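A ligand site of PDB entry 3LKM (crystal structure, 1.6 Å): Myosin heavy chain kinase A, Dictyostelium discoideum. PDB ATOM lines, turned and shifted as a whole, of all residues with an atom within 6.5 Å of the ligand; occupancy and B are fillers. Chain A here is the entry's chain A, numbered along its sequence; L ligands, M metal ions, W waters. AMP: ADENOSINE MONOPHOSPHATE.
An oxygen (O2P) of the ligand lies within salt-bridge range of the side-chain amino group (NZ) of Lys 111 (2.6 Å).
O of Pro 180 sits at hydrogen-bond distance from N6 of the ligand (2.8 Å).
The side-chain carboxylate (OE1) of Glu 179 is in hydrogen-bond range of a nitrogen (N6) of the ligand (2.9 Å).
N of Leu 182 sits at hydrogen-bond distance from N1 of the ligand, 2.9 Å away.
NH2 of Arg 58 lies within salt-bridge range of O2P of the ligand (2.9 Å).
The side-chain carboxylate (OD2) of Asp 232 lies close to an oxygen (O2P) of the ligand.
The side-chain amino group (NZ) of Lys 111 lies within salt-bridge range of the side-chain carboxylate (OE2) of Glu 179 (2.9 Å).
The side-chain carboxylate of Glu 179 sits at hydrogen-bond distance from the side-chain hydroxyl of Thr 231.
The backbone carbonyl oxygen (O) of Glu 179 is in hydrogen-bond range of the backbone NH (N) of Val 109, 2.9 Å away.
The guanidinium group (NH2) of Arg 58 lies within salt-bridge range of the side-chain carboxylate (OD1) of Asp 232 (3.3 Å).
The side-chain amide nitrogen (NE2) of Gln 224 lies within hydrogen-bond range of the backbone carbonyl oxygen (O) of Asp 232, 2.9 Å away.
O of Ala 53 lies within hydrogen-bond range of N of Ala 60, 2.8 Å away.
The backbone NH of Phe 52 lies within hydrogen-bond range of the backbone carbonyl oxygen of Ala 60 (2.8 Å).
N of Thr 231 is in hydrogen-bond range of O of Gln 224 (2.8 Å).
Phe 52 touches the ligand.
Ala 53 touches the ligand (CB to O4', 3.3 Å).
C of Glu 54 touches C5' of the ligand, at 3.5 Å.
N of Gly 55 touches C5' of the ligand (3.5 Å).
Ala 60 touches the ligand (CB to O4', 3.7 Å).
Val 109 touches the ligand (CG2 to N1, 3.8 Å).
Leu 155 touches the ligand (CD1 to N6, 3.6 Å).
Leu 181 touches the ligand (CD1 to C2, 3.8 Å).
Phe 186 touches the ligand (CE1 to N9, 3.7 Å).
Thr 231 touches the ligand.
Hydrophobic or aromatic side chains within 4 Å of the ligand: Phe 52, Ala 53, Ala 60, Val 109, Leu 155, Leu 181, Leu 182 and Phe 186.
Within 4 Å of the ligand: Phe 52, Ala 53, Glu 54, Gly 55, Arg 58, Ala 60, Val 109, Lys 111, Leu 155, Glu 179, Pro 180, Leu 181, Leu 182, Phe 186, Thr 231 and Asp 232.
The nearest printed residue that does not touch the ligand is Gln 224 (4.4 Å).
Water W1 bridges an oxygen (O3') of the ligand (2.7 Å) and the backbone carbonyl oxygen (O) of Glu 54 (3.2 Å).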
ATOM      1  N   PHE A  52       2.263 -19.572 -31.188  1.00  0.00           N
ATOM      2  CA  PHE A  52       2.394 -18.513 -30.184  1.00  0.00           C
ATOM      3  C   PHE A  52       1.989 -18.973 -28.797  1.00  0.00           C
ATOM      4  O   PHE A  52       2.292 -18.301 -27.802  1.00  0.00           O
ATOM      5  CB  PHE A  52       1.607 -17.264 -30.586  1.00  0.00           C
ATOM      6  CG  PHE A  52       0.121 -17.427 -30.506  1.00  0.00           C
ATOM      7  CD1 PHE A  52      -0.572 -17.110 -29.345  1.00  0.00           C
ATOM      8  CD2 PHE A  52      -0.595 -17.881 -31.593  1.00  0.00           C
ATOM      9  CE1 PHE A  52      -1.942 -17.239 -29.269  1.00  0.00           C
ATOM     10  CE2 PHE A  52      -1.983 -18.020 -31.530  1.00  0.00           C
ATOM     11  CZ  PHE A  52      -2.648 -17.692 -30.355  1.00  0.00           C
ATOM     12  N   ALA A  53       1.320 -20.118 -28.730  1.00  0.00           N
ATOM     13  CA  ALA A  53       0.861 -20.664 -27.457  1.00  0.00           C
ATOM     14  C   ALA A  53       0.572 -22.155 -27.609  1.00  0.00           C
ATOM     15  O   ALA A  53       0.518 -22.673 -28.720  1.00  0.00           O
ATOM     16  CB  ALA A  53      -0.378 -19.911 -26.983  1.00  0.00           C
ATOM     17  N   GLU A  54       0.417 -22.852 -26.480  1.00  0.00           N
ATOM     18  CA  GLU A  54       0.051 -24.266 -26.526  1.00  0.00           C
ATOM     19  C   GLU A  54      -0.721 -24.704 -25.294  1.00  0.00           C
ATOM     20  O   GLU A  54      -0.680 -24.055 -24.252  1.00  0.00           O
ATOM     21  CB  GLU A  54       1.289 -25.151 -26.707  1.00  0.00           C
ATOM     22  CG  GLU A  54       2.152 -25.302 -25.464  1.00  0.00           C
ATOM     23  CD  GLU A  54       3.414 -26.086 -25.726  1.00  0.00           C
ATOM     24  OE1 GLU A  54       4.245 -25.615 -26.524  1.00  0.00           O
ATOM     25  OE2 GLU A  54       3.592 -27.180 -25.141  1.00  0.00           O
ATOM     26  N   GLY A  55      -1.435 -25.809 -25.444  1.00  0.00           N
ATOM     27  CA  GLY A  55      -2.130 -26.444 -24.340  1.00  0.00           C
ATOM     28  C   GLY A  55      -1.585 -27.849 -24.195  1.00  0.00           C
ATOM     29  O   GLY A  55      -0.543 -28.178 -24.772  1.00  0.00           O
ATOM     30  N   ALA A  56      -2.288 -28.691 -23.442  1.00  0.00           N
ATOM     31  CA  ALA A  56      -1.869 -30.083 -23.275  1.00  0.00           C
ATOM     32  C   ALA A  56      -1.737 -30.825 -24.594  1.00  0.00           C
ATOM     33  O   ALA A  56      -0.753 -31.532 -24.825  1.00  0.00           O
ATOM     34  CB  ALA A  56      -2.826 -30.822 -22.345  1.00  0.00           C
ATOM     35  N   LEU A  57      -2.729 -30.659 -25.474  1.00  0.00           N
ATOM     36  CA  LEU A  57      -2.823 -31.457 -26.695  1.00  0.00           C
ATOM     37  C   LEU A  57      -2.461 -30.709 -27.976  1.00  0.00           C
ATOM     38  O   LEU A  57      -2.013 -31.314 -28.952  1.00  0.00           O
ATOM     39  CB  LEU A  57      -4.227 -32.056 -26.830  1.00  0.00           C
ATOM     40  CG  LEU A  57      -4.667 -33.088 -25.787  1.00  0.00           C
ATOM     41  CD1 LEU A  57      -6.148 -33.376 -25.923  1.00  0.00           C
ATOM     42  CD2 LEU A  57      -3.868 -34.357 -25.967  1.00  0.00           C
ATOM     43  N   ARG A  58      -2.657 -29.391 -27.979  1.00  0.00           N
ATOM     44  CA  ARG A  58      -2.562 -28.628 -29.229  1.00  0.00           C
ATOM     45  C   ARG A  58      -1.632 -27.422 -29.128  1.00  0.00           C
ATOM     46  O   ARG A  58      -1.340 -26.928 -28.037  1.00  0.00           O
ATOM     47  CB  ARG A  58      -3.951 -28.157 -29.670  1.00  0.00           C
ATOM     48  CG  ARG A  58      -5.000 -29.272 -29.755  1.00  0.00           C
ATOM     49  CD  ARG A  58      -6.307 -28.792 -30.356  1.00  0.00           C
ATOM     50  NE  ARG A  58      -6.933 -27.742 -29.561  1.00  0.00           N
ATOM     51  CZ  ARG A  58      -8.115 -27.191 -29.855  1.00  0.00           C
ATOM     52  NH1 ARG A  58      -8.788 -27.599 -30.927  1.00  0.00           N
ATOM     53  NH2 ARG A  58      -8.622 -26.240 -29.081  1.00  0.00           N
ATOM     54  N   GLU A  59      -1.182 -26.951 -30.289  1.00  0.00           N
ATOM     55  CA  GLU A  59      -0.439 -25.702 -30.396  1.00  0.00           C
ATOM     56  C   GLU A  59      -1.213 -24.714 -31.256  1.00  0.00           C
ATOM     57  O   GLU A  59      -1.891 -25.107 -32.195  1.00  0.00           O
ATOM     58  CB  GLU A  59       0.945 -25.950 -30.993  1.00  0.00           C
ATOM     59  CG  GLU A  59       1.857 -26.742 -30.069  1.00  0.00           C
ATOM     60  CD  GLU A  59       3.233 -27.005 -30.660  1.00  0.00           C
ATOM     61  OE1 GLU A  59       3.319 -27.626 -31.741  1.00  0.00           O
ATOM     62  OE2 GLU A  59       4.240 -26.610 -30.025  1.00  0.00           O
ATOM     63  N   ALA A  60      -1.114 -23.423 -30.921  1.00  0.00           N
ATOM     64  CA  ALA A  60      -1.910 -22.387 -31.571  1.00  0.00           C
ATOM     65  C   ALA A  60      -1.030 -21.449 -32.404  1.00  0.00           C
ATOM     66  O   ALA A  60       0.038 -21.039 -31.959  1.00  0.00           O
ATOM     67  CB  ALA A  60      -2.667 -21.596 -30.522  1.00  0.00           C
ATOM     68  N   HIS A  62      -0.882 -17.979 -35.116  1.00  0.00           N
ATOM     69  CA  HIS A  62      -1.522 -16.801 -35.722  1.00  0.00           C
ATOM     70  C   HIS A  62      -1.657 -17.007 -37.216  1.00  0.00           C
ATOM     71  O   HIS A  62      -0.724 -17.449 -37.892  1.00  0.00           O
ATOM     72  CB  HIS A  62      -0.727 -15.531 -35.452  1.00  0.00           C
ATOM     73  CG  HIS A  62      -0.765 -15.094 -34.024  1.00  0.00           C
ATOM     74  ND1 HIS A  62      -1.930 -14.772 -33.370  1.00  0.00           N
ATOM     75  CD2 HIS A  62       0.235 -14.908 -33.124  1.00  0.00           C
ATOM     76  CE1 HIS A  62      -1.656 -14.415 -32.126  1.00  0.00           C
ATOM     77  NE2 HIS A  62      -0.353 -14.498 -31.955  1.00  0.00           N
ATOM     78  N   VAL A 109      -6.956 -17.795 -35.456  1.00  0.00           N
ATOM     79  CA  VAL A 109      -6.063 -18.746 -34.812  1.00  0.00           C
ATOM     80  C   VAL A 109      -6.252 -20.138 -35.413  1.00  0.00           C
ATOM     81  O   VAL A 109      -7.379 -20.578 -35.633  1.00  0.00           O
ATOM     82  CB  VAL A 109      -6.309 -18.744 -33.277  1.00  0.00           C
ATOM     83  CG1 VAL A 109      -5.546 -19.881 -32.577  1.00  0.00           C
ATOM     84  CG2 VAL A 109      -5.918 -17.402 -32.704  1.00  0.00           C
ATOM     85  N   LYS A 111      -5.123 -24.254 -34.991  1.00  0.00           N
ATOM     86  CA  LYS A 111      -4.609 -25.162 -33.983  1.00  0.00           C
ATOM     87  C   LYS A 111      -4.314 -26.535 -34.569  1.00  0.00           C
ATOM     88  O   LYS A 111      -5.110 -27.080 -35.333  1.00  0.00           O
ATOM     89  CB  LYS A 111      -5.609 -25.288 -32.828  1.00  0.00           C
ATOM     90  CG  LYS A 111      -5.787 -23.959 -32.093  1.00  0.00           C
ATOM     91  CD  LYS A 111      -6.790 -24.063 -30.972  1.00  0.00           C
ATOM     92  CE  LYS A 111      -6.973 -22.700 -30.331  1.00  0.00           C
ATOM     93  NZ  LYS A 111      -8.014 -22.757 -29.266  1.00  0.00           N
ATOM     94  N   LEU A 155     -16.662 -19.217 -28.814  1.00  0.00           N
ATOM     95  CA  LEU A 155     -16.244 -18.945 -30.185  1.00  0.00           C
ATOM     96  C   LEU A 155     -16.716 -20.038 -31.121  1.00  0.00           C
ATOM     97  O   LEU A 155     -16.826 -21.206 -30.740  1.00  0.00           O
ATOM     98  CB  LEU A 155     -14.709 -18.885 -30.283  1.00  0.00           C
ATOM     99  CG  LEU A 155     -14.003 -17.720 -29.599  1.00  0.00           C
ATOM    100  CD1 LEU A 155     -12.504 -17.847 -29.796  1.00  0.00           C
ATOM    101  CD2 LEU A 155     -14.537 -16.402 -30.149  1.00  0.00           C
ATOM    102  N   GLU A 179     -10.282 -20.898 -35.399  1.00  0.00           N
ATOM    103  CA  GLU A 179     -11.261 -20.142 -34.629  1.00  0.00           C
ATOM    104  C   GLU A 179     -10.832 -18.686 -34.603  1.00  0.00           C
ATOM    105  O   GLU A 179      -9.704 -18.378 -34.931  1.00  0.00           O
ATOM    106  CB  GLU A 179     -11.327 -20.683 -33.203  1.00  0.00           C
ATOM    107  CG  GLU A 179     -10.007 -20.625 -32.472  1.00  0.00           C
ATOM    108  CD  GLU A 179     -10.049 -21.400 -31.164  1.00  0.00           C
ATOM    109  OE1 GLU A 179     -10.047 -20.759 -30.090  1.00  0.00           O
ATOM    110  OE2 GLU A 179     -10.098 -22.654 -31.221  1.00  0.00           O
ATOM    111  N   PRO A 180     -11.748 -17.805 -34.195  1.00  0.00           N
ATOM    112  CA  PRO A 180     -11.403 -16.390 -34.104  1.00  0.00           C
ATOM    113  C   PRO A 180     -10.298 -16.117 -33.093  1.00  0.00           C
ATOM    114  O   PRO A 180     -10.089 -16.907 -32.175  1.00  0.00           O
ATOM    115  CB  PRO A 180     -12.718 -15.726 -33.659  1.00  0.00           C
ATOM    116  CG  PRO A 180     -13.789 -16.686 -34.112  1.00  0.00           C
ATOM    117  CD  PRO A 180     -13.182 -18.046 -33.911  1.00  0.00           C
ATOM    118  N   LEU A 181      -9.590 -15.011 -33.271  1.00  0.00           N
ATOM    119  CA  LEU A 181      -8.572 -14.588 -32.329  1.00  0.00           C
ATOM    120  C   LEU A 181      -9.215 -13.871 -31.142  1.00  0.00           C
ATOM    121  O   LEU A 181      -9.998 -12.948 -31.332  1.00  0.00           O
ATOM    122  CB  LEU A 181      -7.582 -13.648 -33.028  1.00  0.00           C
ATOM    123  CG  LEU A 181      -6.527 -12.973 -32.135  1.00  0.00           C
ATOM    124  CD1 LEU A 181      -5.559 -13.998 -31.575  1.00  0.00           C
ATOM    125  CD2 LEU A 181      -5.766 -11.887 -32.930  1.00  0.00           C
ATOM    126  N   LEU A 182      -8.889 -14.313 -29.934  1.00  0.00           N
ATOM    127  CA  LEU A 182      -9.296 -13.614 -28.724  1.00  0.00           C
ATOM    128  C   LEU A 182      -8.286 -12.526 -28.413  1.00  0.00           C
ATOM    129  O   LEU A 182      -7.074 -12.772 -28.371  1.00  0.00           O
ATOM    130  CB  LEU A 182      -9.367 -14.558 -27.529  1.00  0.00           C
ATOM    131  CG  LEU A 182     -10.478 -15.612 -27.577  1.00  0.00           C
ATOM    132  CD1 LEU A 182     -10.281 -16.631 -26.455  1.00  0.00           C
ATOM    133  CD2 LEU A 182     -11.839 -14.943 -27.490  1.00  0.00           C
ATOM    134  N   VAL A 183      -8.792 -11.311 -28.203  1.00  0.00           N
ATOM    135  CA  VAL A 183      -7.931 -10.190 -27.851  1.00  0.00           C
ATOM    136  C   VAL A 183      -8.124  -9.856 -26.368  1.00  0.00           C
ATOM    137  O   VAL A 183      -9.240  -9.561 -25.939  1.00  0.00           O
ATOM    138  CB  VAL A 183      -8.227  -8.977 -28.728  1.00  0.00           C
ATOM    139  CG1 VAL A 183      -7.290  -7.828 -28.381  1.00  0.00           C
ATOM    140  CG2 VAL A 183      -8.097  -9.361 -30.194  1.00  0.00           C
ATOM    141  N   PHE A 186      -6.111 -13.978 -21.670  1.00  0.00           N
ATOM    142  CA  PHE A 186      -6.682 -15.319 -21.754  1.00  0.00           C
ATOM    143  C   PHE A 186      -6.507 -16.005 -20.403  1.00  0.00           C
ATOM    144  O   PHE A 186      -5.390 -16.153 -19.917  1.00  0.00           O
ATOM    145  CB  PHE A 186      -5.975 -16.115 -22.845  1.00  0.00           C
ATOM    146  CG  PHE A 186      -6.628 -17.435 -23.172  1.00  0.00           C
ATOM    147  CD1 PHE A 186      -7.322 -17.602 -24.379  1.00  0.00           C
ATOM    148  CD2 PHE A 186      -6.547 -18.522 -22.303  1.00  0.00           C
ATOM    149  CE1 PHE A 186      -7.924 -18.810 -24.691  1.00  0.00           C
ATOM    150  CE2 PHE A 186      -7.149 -19.731 -22.614  1.00  0.00           C
ATOM    151  CZ  PHE A 186      -7.826 -19.879 -23.805  1.00  0.00           C
ATOM    152  N   LYS A 188      -7.843 -19.357 -17.844  1.00  0.00           N
ATOM    153  CA  LYS A 188      -8.545 -20.614 -17.636  1.00  0.00           C
ATOM    154  C   LYS A 188      -9.214 -20.616 -16.272  1.00  0.00           C
ATOM    155  O   LYS A 188      -8.571 -20.321 -15.260  1.00  0.00           O
ATOM    156  CB  LYS A 188      -7.553 -21.774 -17.722  1.00  0.00           C
ATOM    157  CG  LYS A 188      -8.212 -23.146 -17.707  1.00  0.00           C
ATOM    158  CD  LYS A 188      -7.162 -24.223 -17.958  1.00  0.00           C
ATOM    159  CE  LYS A 188      -7.808 -25.516 -18.383  1.00  0.00           C
ATOM    160  NZ  LYS A 188      -6.881 -26.368 -19.185  1.00  0.00           N
ATOM    161  N   GLN A 224     -12.626 -21.378 -20.378  1.00  0.00           N
ATOM    162  CA  GLN A 224     -11.434 -20.532 -20.547  1.00  0.00           C
ATOM    163  C   GLN A 224     -11.589 -19.571 -21.725  1.00  0.00           C
ATOM    164  O   GLN A 224     -12.261 -19.882 -22.708  1.00  0.00           O
ATOM    165  CB  GLN A 224     -10.217 -21.406 -20.766  1.00  0.00           C
ATOM    166  CG  GLN A 224     -10.316 -22.288 -21.996  1.00  0.00           C
ATOM    167  CD  GLN A 224      -9.157 -23.243 -22.113  1.00  0.00           C
ATOM    168  OE1 GLN A 224      -8.024 -22.908 -21.751  1.00  0.00           O
ATOM    169  NE2 GLN A 224      -9.423 -24.440 -22.607  1.00  0.00           N
ATOM    170  N   VAL A 226     -11.296 -15.057 -22.831  1.00  0.00           N
ATOM    171  CA  VAL A 226     -11.144 -13.669 -22.411  1.00  0.00           C
ATOM    172  C   VAL A 226     -12.479 -13.179 -21.889  1.00  0.00           C
ATOM    173  O   VAL A 226     -13.488 -13.162 -22.609  1.00  0.00           O
ATOM    174  CB  VAL A 226     -10.635 -12.793 -23.557  1.00  0.00           C
ATOM    175  CG1 VAL A 226     -10.622 -11.311 -23.138  1.00  0.00           C
ATOM    176  CG2 VAL A 226      -9.264 -13.260 -24.008  1.00  0.00           C
ATOM    177  N   THR A 231     -13.361 -20.397 -25.278  1.00  0.00           N
ATOM    178  CA  THR A 231     -13.009 -21.313 -26.340  1.00  0.00           C
ATOM    179  C   THR A 231     -12.401 -22.598 -25.782  1.00  0.00           C
ATOM    180  O   THR A 231     -12.069 -22.673 -24.601  1.00  0.00           O
ATOM    181  CB  THR A 231     -12.065 -20.660 -27.365  1.00  0.00           C
ATOM    182  OG1 THR A 231     -12.039 -21.444 -28.566  1.00  0.00           O
ATOM    183  CG2 THR A 231     -10.653 -20.535 -26.795  1.00  0.00           C
ATOM    184  N   ASP A 232     -12.290 -23.601 -26.641  1.00  0.00           N
ATOM    185  CA  ASP A 232     -11.791 -24.937 -26.266  1.00  0.00           C
ATOM    186  C   ASP A 232     -12.326 -25.464 -24.939  1.00  0.00           C
ATOM    187  O   ASP A 232     -11.558 -25.846 -24.051  1.00  0.00           O
ATOM    188  CB  ASP A 232     -10.258 -24.986 -26.276  1.00  0.00           C
ATOM    189  CG  ASP A 232      -9.743 -26.394 -26.162  1.00  0.00           C
ATOM    190  OD1 ASP A 232     -10.473 -27.334 -26.561  1.00  0.00           O
ATOM    191  OD2 ASP A 232      -8.603 -26.560 -25.673  1.00  0.00           O
HETATM  192  P   AMP L   1      -5.916 -24.691 -26.719  1.00  0.00           P
HETATM  193  O1P AMP L   1      -5.889 -24.902 -25.232  1.00  0.00           O
HETATM  194  O2P AMP L   1      -7.264 -24.321 -27.305  1.00  0.00           O
HETATM  195  O3P AMP L   1      -5.204 -25.765 -27.495  1.00  0.00           O
HETATM  196  O5' AMP L   1      -5.025 -23.352 -26.907  1.00  0.00           O
HETATM  197  C5' AMP L   1      -3.726 -23.279 -26.340  1.00  0.00           C
HETATM  198  C4' AMP L   1      -3.406 -21.869 -25.867  1.00  0.00           C
HETATM  199  O4' AMP L   1      -3.535 -20.948 -26.954  1.00  0.00           O
HETATM  200  C3' AMP L   1      -4.330 -21.337 -24.786  1.00  0.00           C
HETATM  201  O3' AMP L   1      -3.902 -21.732 -23.482  1.00  0.00           O
HETATM  202  C2' AMP L   1      -4.271 -19.836 -24.981  1.00  0.00           C
HETATM  203  O2' AMP L   1      -3.072 -19.319 -24.407  1.00  0.00           O
HETATM  204  C1' AMP L   1      -4.127 -19.725 -26.491  1.00  0.00           C
HETATM  205  N9  AMP L   1      -5.395 -19.619 -27.230  1.00  0.00           N
HETATM  206  C8  AMP L   1      -6.246 -20.633 -27.490  1.00  0.00           C
HETATM  207  N7  AMP L   1      -7.288 -20.201 -28.239  1.00  0.00           N
HETATM  208  C5  AMP L   1      -7.072 -18.894 -28.501  1.00  0.00           C
HETATM  209  C6  AMP L   1      -7.798 -17.846 -29.235  1.00  0.00           C
HETATM  210  N6  AMP L   1      -8.947 -18.130 -29.887  1.00  0.00           N
HETATM  211  N1  AMP L   1      -7.246 -16.618 -29.265  1.00  0.00           N
HETATM  212  C2  AMP L   1      -6.086 -16.338 -28.626  1.00  0.00           C
HETATM  213  N3  AMP L   1      -5.364 -17.244 -27.926  1.00  0.00           N
HETATM  214  C4  AMP L   1      -5.828 -18.519 -27.843  1.00  0.00           C
HETATM  215 MG    MG M   1      -5.708 -23.665 -22.876  1.00  0.00          MG
HETATM  216  O   HOH W   1      -1.410 -21.360 -22.632  1.00  0.00           O
HETATM  217  O   HOH W   2      -3.879 -15.522 -26.228  1.00  0.00           O
HETATM  218  O   HOH W   3      -2.581 -16.742 -24.223  1.00  0.00           O
